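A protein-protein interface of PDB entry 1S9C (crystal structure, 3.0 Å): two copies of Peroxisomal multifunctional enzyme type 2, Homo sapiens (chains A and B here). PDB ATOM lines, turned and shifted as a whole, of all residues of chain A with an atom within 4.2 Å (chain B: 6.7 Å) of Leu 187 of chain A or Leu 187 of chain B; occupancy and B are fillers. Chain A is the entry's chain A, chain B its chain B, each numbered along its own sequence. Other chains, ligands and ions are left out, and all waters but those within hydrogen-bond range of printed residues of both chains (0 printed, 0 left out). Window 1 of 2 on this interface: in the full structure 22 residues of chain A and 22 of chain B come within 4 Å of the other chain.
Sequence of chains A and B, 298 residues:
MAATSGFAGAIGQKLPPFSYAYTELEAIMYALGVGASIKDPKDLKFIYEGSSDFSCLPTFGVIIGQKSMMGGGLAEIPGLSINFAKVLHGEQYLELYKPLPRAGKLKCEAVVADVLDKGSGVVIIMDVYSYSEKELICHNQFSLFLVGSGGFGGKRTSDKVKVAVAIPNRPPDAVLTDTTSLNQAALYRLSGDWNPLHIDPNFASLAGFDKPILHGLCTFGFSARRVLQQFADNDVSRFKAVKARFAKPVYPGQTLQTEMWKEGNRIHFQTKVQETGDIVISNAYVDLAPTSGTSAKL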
ATOM      1  N   LEU A  32      13.910 -16.897   5.259  1.00  0.00           N
ATOM      2  CA  LEU A  32      13.453 -17.951   6.148  1.00  0.00           C
ATOM      3  C   LEU A  32      12.425 -18.803   5.434  1.00  0.00           C
ATOM      4  O   LEU A  32      12.546 -20.028   5.395  1.00  0.00           O
ATOM      5  CB  LEU A  32      12.851 -17.364   7.421  1.00  0.00           C
ATOM      6  CG  LEU A  32      13.883 -16.817   8.418  1.00  0.00           C
ATOM      7  CD1 LEU A  32      13.198 -16.220   9.644  1.00  0.00           C
ATOM      8  CD2 LEU A  32      14.796 -17.947   8.826  1.00  0.00           C
ATOM      9  N   GLY A  33      11.423 -18.160   4.849  1.00  0.00           N
ATOM     10  CA  GLY A  33      10.394 -18.906   4.159  1.00  0.00           C
ATOM     11  C   GLY A  33      10.924 -19.666   2.967  1.00  0.00           C
ATOM     12  O   GLY A  33      10.238 -20.514   2.391  1.00  0.00           O
ATOM     13  N   ASN A 183       5.053 -26.217   7.893  1.00  0.00           N
ATOM     14  CA  ASN A 183       4.529 -24.857   7.770  1.00  0.00           C
ATOM     15  C   ASN A 183       5.264 -24.019   6.713  1.00  0.00           C
ATOM     16  O   ASN A 183       5.101 -22.806   6.647  1.00  0.00           O
ATOM     17  CB  ASN A 183       4.654 -24.138   9.098  1.00  0.00           C
ATOM     18  CG  ASN A 183       3.788 -24.734  10.164  1.00  0.00           C
ATOM     19  OD1 ASN A 183       2.608 -24.408  10.265  1.00  0.00           O
ATOM     20  ND2 ASN A 183       4.367 -25.617  10.980  1.00  0.00           N
ATOM     21  N   GLN A 184       6.088 -24.653   5.899  1.00  0.00           N
ATOM     22  CA  GLN A 184       6.817 -23.926   4.890  1.00  0.00           C
ATOM     23  C   GLN A 184       5.896 -22.973   4.146  1.00  0.00           C
ATOM     24  O   GLN A 184       6.194 -21.792   4.020  1.00  0.00           O
ATOM     25  CB  GLN A 184       7.451 -24.888   3.905  1.00  0.00           C
ATOM     26  CG  GLN A 184       8.712 -24.357   3.253  1.00  0.00           C
ATOM     27  CD  GLN A 184       9.811 -24.099   4.271  1.00  0.00           C
ATOM     28  OE1 GLN A 184      10.123 -24.961   5.085  1.00  0.00           O
ATOM     29  NE2 GLN A 184      10.403 -22.907   4.225  1.00  0.00           N
ATOM     30  N   ALA A 185       4.774 -23.478   3.651  1.00  0.00           N
ATOM     31  CA  ALA A 185       3.840 -22.636   2.916  1.00  0.00           C
ATOM     32  C   ALA A 185       3.257 -21.534   3.806  1.00  0.00           C
ATOM     33  O   ALA A 185       3.119 -20.380   3.388  1.00  0.00           O
ATOM     34  CB  ALA A 185       2.728 -23.481   2.343  1.00  0.00           C
ATOM     35  N   ALA A 186       2.923 -21.886   5.036  1.00  0.00           N
ATOM     36  CA  ALA A 186       2.347 -20.915   5.949  1.00  0.00           C
ATOM     37  C   ALA A 186       3.276 -19.723   6.170  1.00  0.00           C
ATOM     38  O   ALA A 186       2.809 -18.602   6.425  1.00  0.00           O
ATOM     39  CB  ALA A 186       2.021 -21.585   7.286  1.00  0.00           C
ATOM     40  N   LEU A 187       4.584 -19.961   6.080  1.00  0.00           N
ATOM     41  CA  LEU A 187       5.555 -18.893   6.273  1.00  0.00           C
ATOM     42  C   LEU A 187       5.874 -18.159   4.971  1.00  0.00           C
ATOM     43  O   LEU A 187       5.887 -16.932   4.917  1.00  0.00           O
ATOM     44  CB  LEU A 187       6.845 -19.448   6.865  1.00  0.00           C
ATOM     45  CG  LEU A 187       7.955 -18.399   7.027  1.00  0.00           C
ATOM     46  CD1 LEU A 187       7.499 -17.293   7.969  1.00  0.00           C
ATOM     47  CD2 LEU A 187       9.214 -19.057   7.571  1.00  0.00           C
ATOM     48  N   TYR A 188       6.131 -18.917   3.916  1.00  0.00           N
ATOM     49  CA  TYR A 188       6.448 -18.318   2.640  1.00  0.00           C
ATOM     50  C   TYR A 188       5.352 -17.396   2.134  1.00  0.00           C
ATOM     51  O   TYR A 188       5.647 -16.371   1.528  1.00  0.00           O
ATOM     52  CB  TYR A 188       6.714 -19.395   1.594  1.00  0.00           C
ATOM     53  CG  TYR A 188       7.175 -18.819   0.280  1.00  0.00           C
ATOM     54  CD1 TYR A 188       8.441 -18.273   0.142  1.00  0.00           C
ATOM     55  CD2 TYR A 188       6.315 -18.754  -0.818  1.00  0.00           C
ATOM     56  CE1 TYR A 188       8.842 -17.670  -1.061  1.00  0.00           C
ATOM     57  CE2 TYR A 188       6.701 -18.149  -2.019  1.00  0.00           C
ATOM     58  CZ  TYR A 188       7.959 -17.613  -2.132  1.00  0.00           C
ATOM     59  OH  TYR A 188       8.338 -17.027  -3.310  1.00  0.00           O
ATOM     60  N   ARG A 189       4.088 -17.751   2.366  1.00  0.00           N
ATOM     61  CA  ARG A 189       2.988 -16.918   1.882  1.00  0.00           C
ATOM     62  C   ARG A 189       3.026 -15.493   2.468  1.00  0.00           C
ATOM     63  O   ARG A 189       2.540 -14.543   1.840  1.00  0.00           O
ATOM     64  CB  ARG A 189       1.639 -17.596   2.158  1.00  0.00           C
ATOM     65  CG  ARG A 189       1.310 -17.815   3.626  1.00  0.00           C
ATOM     66  CD  ARG A 189       0.083 -18.713   3.757  1.00  0.00           C
ATOM     67  NE  ARG A 189      -1.061 -18.185   3.013  1.00  0.00           N
ATOM     68  CZ  ARG A 189      -1.996 -17.396   3.538  1.00  0.00           C
ATOM     69  NH1 ARG A 189      -1.924 -17.052   4.817  1.00  0.00           N
ATOM     70  NH2 ARG A 189      -2.989 -16.940   2.780  1.00  0.00           N
ATOM     71  N   LEU A 190       3.633 -15.337   3.645  1.00  0.00           N
ATOM     72  CA  LEU A 190       3.733 -14.022   4.271  1.00  0.00           C
ATOM     73  C   LEU A 190       4.536 -13.079   3.411  1.00  0.00           C
ATOM     74  O   LEU A 190       4.653 -11.901   3.727  1.00  0.00           O
ATOM     75  CB  LEU A 190       4.413 -14.101   5.634  1.00  0.00           C
ATOM     76  CG  LEU A 190       3.729 -14.953   6.693  1.00  0.00           C
ATOM     77  CD1 LEU A 190       4.434 -14.777   8.026  1.00  0.00           C
ATOM     78  CD2 LEU A 190       2.277 -14.529   6.799  1.00  0.00           C
ATOM     79  N   MET B  29       2.588 -13.767  11.754  1.00  0.00           N
ATOM     80  CA  MET B  29       4.029 -13.860  11.919  1.00  0.00           C
ATOM     81  C   MET B  29       4.339 -14.130  13.394  1.00  0.00           C
ATOM     82  O   MET B  29       5.219 -14.921  13.719  1.00  0.00           O
ATOM     83  CB  MET B  29       4.691 -12.559  11.468  1.00  0.00           C
ATOM     84  CG  MET B  29       6.066 -12.745  10.843  1.00  0.00           C
ATOM     85  SD  MET B  29       6.816 -11.204  10.217  1.00  0.00           S
ATOM     86  CE  MET B  29       5.350 -10.115   9.976  1.00  0.00           C
ATOM     87  N   TYR B  30       3.615 -13.472  14.291  1.00  0.00           N
ATOM     88  CA  TYR B  30       3.847 -13.687  15.705  1.00  0.00           C
ATOM     89  C   TYR B  30       3.482 -15.118  16.052  1.00  0.00           C
ATOM     90  O   TYR B  30       4.252 -15.826  16.694  1.00  0.00           O
ATOM     91  CB  TYR B  30       3.003 -12.742  16.553  1.00  0.00           C
ATOM     92  CG  TYR B  30       3.112 -13.022  18.042  1.00  0.00           C
ATOM     93  CD1 TYR B  30       4.226 -12.625  18.761  1.00  0.00           C
ATOM     94  CD2 TYR B  30       2.095 -13.685  18.733  1.00  0.00           C
ATOM     95  CE1 TYR B  30       4.329 -12.868  20.128  1.00  0.00           C
ATOM     96  CE2 TYR B  30       2.194 -13.938  20.102  1.00  0.00           C
ATOM     97  CZ  TYR B  30       3.316 -13.523  20.787  1.00  0.00           C
ATOM     98  OH  TYR B  30       3.450 -13.781  22.131  1.00  0.00           O
ATOM     99  N   ALA B  31       2.297 -15.537  15.628  1.00  0.00           N
ATOM    100  CA  ALA B  31       1.820 -16.878  15.910  1.00  0.00           C
ATOM    101  C   ALA B  31       2.822 -17.949  15.479  1.00  0.00           C
ATOM    102  O   ALA B  31       3.111 -18.892  16.236  1.00  0.00           O
ATOM    103  CB  ALA B  31       0.488 -17.104  15.225  1.00  0.00           C
ATOM    104  N   LEU B  32       3.347 -17.821  14.265  1.00  0.00           N
ATOM    105  CA  LEU B  32       4.309 -18.797  13.793  1.00  0.00           C
ATOM    106  C   LEU B  32       5.545 -18.766  14.677  1.00  0.00           C
ATOM    107  O   LEU B  32       5.973 -19.795  15.186  1.00  0.00           O
ATOM    108  CB  LEU B  32       4.684 -18.517  12.343  1.00  0.00           C
ATOM    109  CG  LEU B  32       3.619 -18.928  11.331  1.00  0.00           C
ATOM    110  CD1 LEU B  32       4.055 -18.599   9.915  1.00  0.00           C
ATOM    111  CD2 LEU B  32       3.376 -20.401  11.483  1.00  0.00           C
ATOM    112  N   GLY B  33       6.103 -17.579  14.879  1.00  0.00           N
ATOM    113  CA  GLY B  33       7.296 -17.455  15.694  1.00  0.00           C
ATOM    114  C   GLY B  33       7.078 -17.852  17.134  1.00  0.00           C
ATOM    115  O   GLY B  33       8.034 -17.986  17.902  1.00  0.00           O
ATOM    116  N   VAL B  34       5.824 -18.053  17.511  1.00  0.00           N
ATOM    117  CA  VAL B  34       5.540 -18.425  18.883  1.00  0.00           C
ATOM    118  C   VAL B  34       5.082 -19.884  19.030  1.00  0.00           C
ATOM    119  O   VAL B  34       4.708 -20.300  20.114  1.00  0.00           O
ATOM    120  CB  VAL B  34       4.519 -17.415  19.525  1.00  0.00           C
ATOM    121  CG1 VAL B  34       3.100 -17.979  19.540  1.00  0.00           C
ATOM    122  CG2 VAL B  34       4.982 -17.043  20.907  1.00  0.00           C
ATOM    123  N   ILE B  47      -3.077 -18.989  12.004  1.00  0.00           N
ATOM    124  CA  ILE B  47      -2.134 -18.901  10.906  1.00  0.00           C
ATOM    125  C   ILE B  47      -2.731 -18.462   9.577  1.00  0.00           C
ATOM    126  O   ILE B  47      -2.033 -17.902   8.740  1.00  0.00           O
ATOM    127  CB  ILE B  47      -1.472 -20.258  10.690  1.00  0.00           C
ATOM    128  CG1 ILE B  47      -0.930 -20.799  12.018  1.00  0.00           C
ATOM    129  CG2 ILE B  47      -0.356 -20.132   9.691  1.00  0.00           C
ATOM    130  CD1 ILE B  47      -0.317 -22.191  11.869  1.00  0.00           C
ATOM    131  N   ASN B 183      15.750 -22.163  14.411  1.00  0.00           N
ATOM    132  CA  ASN B 183      15.561 -20.786  13.961  1.00  0.00           C
ATOM    133  C   ASN B 183      14.449 -20.058  14.696  1.00  0.00           C
ATOM    134  O   ASN B 183      14.020 -18.993  14.271  1.00  0.00           O
ATOM    135  CB  ASN B 183      15.228 -20.765  12.481  1.00  0.00           C
ATOM    136  CG  ASN B 183      16.373 -21.217  11.627  1.00  0.00           C
ATOM    137  OD1 ASN B 183      17.261 -20.439  11.304  1.00  0.00           O
ATOM    138  ND2 ASN B 183      16.368 -22.491  11.257  1.00  0.00           N
ATOM    139  N   GLN B 184      13.977 -20.624  15.795  1.00  0.00           N
ATOM    140  CA  GLN B 184      12.890 -20.001  16.543  1.00  0.00           C
ATOM    141  C   GLN B 184      13.154 -18.520  16.771  1.00  0.00           C
ATOM    142  O   GLN B 184      12.309 -17.680  16.468  1.00  0.00           O
ATOM    143  CB  GLN B 184      12.689 -20.702  17.888  1.00  0.00           C
ATOM    144  CG  GLN B 184      11.262 -20.631  18.398  1.00  0.00           C
ATOM    145  CD  GLN B 184      10.276 -21.316  17.448  1.00  0.00           C
ATOM    146  OE1 GLN B 184      10.470 -22.477  17.069  1.00  0.00           O
ATOM    147  NE2 GLN B 184       9.217 -20.601  17.067  1.00  0.00           N
ATOM    148  N   ALA B 185      14.334 -18.203  17.293  1.00  0.00           N
ATOM    149  CA  ALA B 185      14.706 -16.820  17.559  1.00  0.00           C
ATOM    150  C   ALA B 185      14.779 -16.011  16.272  1.00  0.00           C
ATOM    151  O   ALA B 185      14.323 -14.880  16.208  1.00  0.00           O
ATOM    152  CB  ALA B 185      16.035 -16.779  18.255  1.00  0.00           C
ATOM    153  N   ALA B 186      15.362 -16.601  15.240  1.00  0.00           N
ATOM    154  CA  ALA B 186      15.490 -15.913  13.975  1.00  0.00           C
ATOM    155  C   ALA B 186      14.134 -15.467  13.449  1.00  0.00           C
ATOM    156  O   ALA B 186      14.036 -14.451  12.770  1.00  0.00           O
ATOM    157  CB  ALA B 186      16.178 -16.817  12.961  1.00  0.00           C
ATOM    158  N   LEU B 187      13.085 -16.220  13.764  1.00  0.00           N
ATOM    159  CA  LEU B 187      11.747 -15.884  13.284  1.00  0.00           C
ATOM    160  C   LEU B 187      11.025 -14.965  14.235  1.00  0.00           C
ATOM    161  O   LEU B 187      10.428 -13.976  13.829  1.00  0.00           O
ATOM    162  CB  LEU B 187      10.893 -17.144  13.088  1.00  0.00           C
ATOM    163  CG  LEU B 187       9.452 -16.903  12.610  1.00  0.00           C
ATOM    164  CD1 LEU B 187       9.438 -16.201  11.265  1.00  0.00           C
ATOM    165  CD2 LEU B 187       8.734 -18.222  12.491  1.00  0.00           C
ATOM    166  N   TYR B 188      11.073 -15.301  15.511  1.00  0.00           N
ATOM    167  CA  TYR B 188      10.387 -14.488  16.506  1.00  0.00           C
ATOM    168  C   TYR B 188      10.867 -13.041  16.534  1.00  0.00           C
ATOM    169  O   TYR B 188      10.083 -12.133  16.763  1.00  0.00           O
ATOM    170  CB  TYR B 188      10.540 -15.095  17.901  1.00  0.00           C
ATOM    171  CG  TYR B 188       9.756 -14.340  18.935  1.00  0.00           C
ATOM    172  CD1 TYR B 188       8.378 -14.427  18.985  1.00  0.00           C
ATOM    173  CD2 TYR B 188      10.392 -13.510  19.849  1.00  0.00           C
ATOM    174  CE1 TYR B 188       7.643 -13.702  19.927  1.00  0.00           C
ATOM    175  CE2 TYR B 188       9.671 -12.780  20.796  1.00  0.00           C
ATOM    176  CZ  TYR B 188       8.292 -12.876  20.839  1.00  0.00           C
ATOM    177  OH  TYR B 188       7.578 -12.166  21.800  1.00  0.00           O
ATOM    178  N   ARG B 189      12.154 -12.823  16.305  1.00  0.00           N
ATOM    179  CA  ARG B 189      12.677 -11.475  16.336  1.00  0.00           C
ATOM    180  C   ARG B 189      12.011 -10.591  15.292  1.00  0.00           C
ATOM    181  O   ARG B 189      11.898  -9.378  15.493  1.00  0.00           O
ATOM    182  CB  ARG B 189      14.204 -11.476  16.168  1.00  0.00           C
ATOM    183  CG  ARG B 189      14.737 -12.038  14.868  1.00  0.00           C
ATOM    184  CD  ARG B 189      16.253 -12.257  14.983  1.00  0.00           C
ATOM    185  NE  ARG B 189      16.952 -11.019  15.323  1.00  0.00           N
ATOM    186  CZ  ARG B 189      17.450 -10.159  14.432  1.00  0.00           C
ATOM    187  NH1 ARG B 189      17.350 -10.393  13.134  1.00  0.00           N
ATOM    188  NH2 ARG B 189      18.023  -9.037  14.838  1.00  0.00           N
ATOM    189  N   LEU B 190      11.540 -11.188  14.201  1.00  0.00           N
ATOM    190  CA  LEU B 190      10.876 -10.417  13.152  1.00  0.00           C
ATOM    191  C   LEU B 190       9.648  -9.721  13.688  1.00  0.00           C
ATOM    192  O   LEU B 190       9.006  -8.962  12.979  1.00  0.00           O
ATOM    193  CB  LEU B 190      10.443 -11.304  11.988  1.00  0.00           C
ATOM    194  CG  LEU B 190      11.540 -12.029  11.219  1.00  0.00           C
ATOM    195  CD1 LEU B 190      10.944 -12.711  10.010  1.00  0.00           C
ATOM    196  CD2 LEU B 190      12.612 -11.039  10.794  1.00  0.00           C
ATOM    197  N   SER B 191       9.307  -9.990  14.936  1.00  0.00           N
ATOM    198  CA  SER B 191       8.143  -9.363  15.527  1.00  0.00           C
ATOM    199  C   SER B 191       8.495  -8.125  16.335  1.00  0.00           C
ATOM    200  O   SER B 191       7.661  -7.600  17.071  1.00  0.00           O
ATOM    201  CB  SER B 191       7.379 -10.364  16.394  1.00  0.00           C
ATOM    202  OG  SER B 191       6.515 -11.153  15.593  1.00  0.00           O
ATOM    203  N   HIS B 215      14.220 -15.492  22.905  1.00  0.00           N
ATOM    204  CA  HIS B 215      13.578 -14.389  23.621  1.00  0.00           C
ATOM    205  C   HIS B 215      12.693 -14.907  24.761  1.00  0.00           C
ATOM    206  O   HIS B 215      11.929 -15.848  24.577  1.00  0.00           O
ATOM    207  CB  HIS B 215      12.694 -13.558  22.681  1.00  0.00           C
ATOM    208  CG  HIS B 215      13.397 -13.050  21.468  1.00  0.00           C
ATOM    209  ND1 HIS B 215      14.002 -13.885  20.555  1.00  0.00           N
ATOM    210  CD2 HIS B 215      13.537 -11.794  20.984  1.00  0.00           C
ATOM    211  CE1 HIS B 215      14.481 -13.165  19.556  1.00  0.00           C
ATOM    212  NE2 HIS B 215      14.212 -11.893  19.792  1.00  0.00           N
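Printed residues of chain A that touch a printed residue of chain B: Leu 32, Ala 186, Leu 187 and Leu 190.
Hydrophobic or aromatic side chains of chain A within 4 Å of the printed part of chain B: Leu 32, Ala 186, Leu 187 and Leu 190.
Among the printed residues, no Asp or Glu carboxylate lies within 4 Å of a Lys or Arg side-chain nitrogen of the other chain.
Leu 32 of chain A touches Ala 186 of chain B, and with the chains exchanged Ala 186 of chain A touches Leu 32 of chain B.
Leu 32 of chain A touches Leu 187 of chain B, and with the chains exchanged Leu 187 of chain A touches Leu 32 of chain B.
Leu 187 of chain A touches its own counterpart, Leu 187 of chain B.
10 positions are printed for both chains.
Of the 7 pairs that touch across the chains among the printed residues, 5 have their exchanged pair printed and touching as well.
Of chain B, only Leu 32 and Leu 187 come within 4 Å of Leu 187 of chain A.
Leu 187 of chain B touches two residues of chain A.
Of the printed residues of chain B, Ala 186 of chain A touches Leu 32 and Ile 47.
Of the printed residues of chain B, Leu 190 of chain A touches Met 29.
Printed residues of chain A within 4 Å of Leu 32 of chain B: Ala 186 (3.7 Å) and Leu 187 (3.9 Å).
Of the printed residues of chain A, Met 29 of chain B touches Leu 190 (3.8 Å).
Leu 190 of chain B touches none of the printed residues of chain A.
The nearest printed residue of chain A that does not touch Leu 187 of chain B is Leu 190 of chain A (6.1 Å).
Leu 32 of chain A touches Ala 186 of chain B (CD1 to O, 3.7 Å).
Leu 32 of chain A touches Leu 187 of chain B.
Leu 32 of chain B touches Ala 186 of chain A (CD1 to O, 3.7 Å).
Ala 186 of chain A touches Ile 47 of chain B.
Leu 187 of chain A touches Leu 32 of chain B.
Leu 187 of chain B touches Leu 187 of chain A (CD1 to CD1, 3.98 Å).
Met 29 of chain B touches Leu 190 of chain A.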
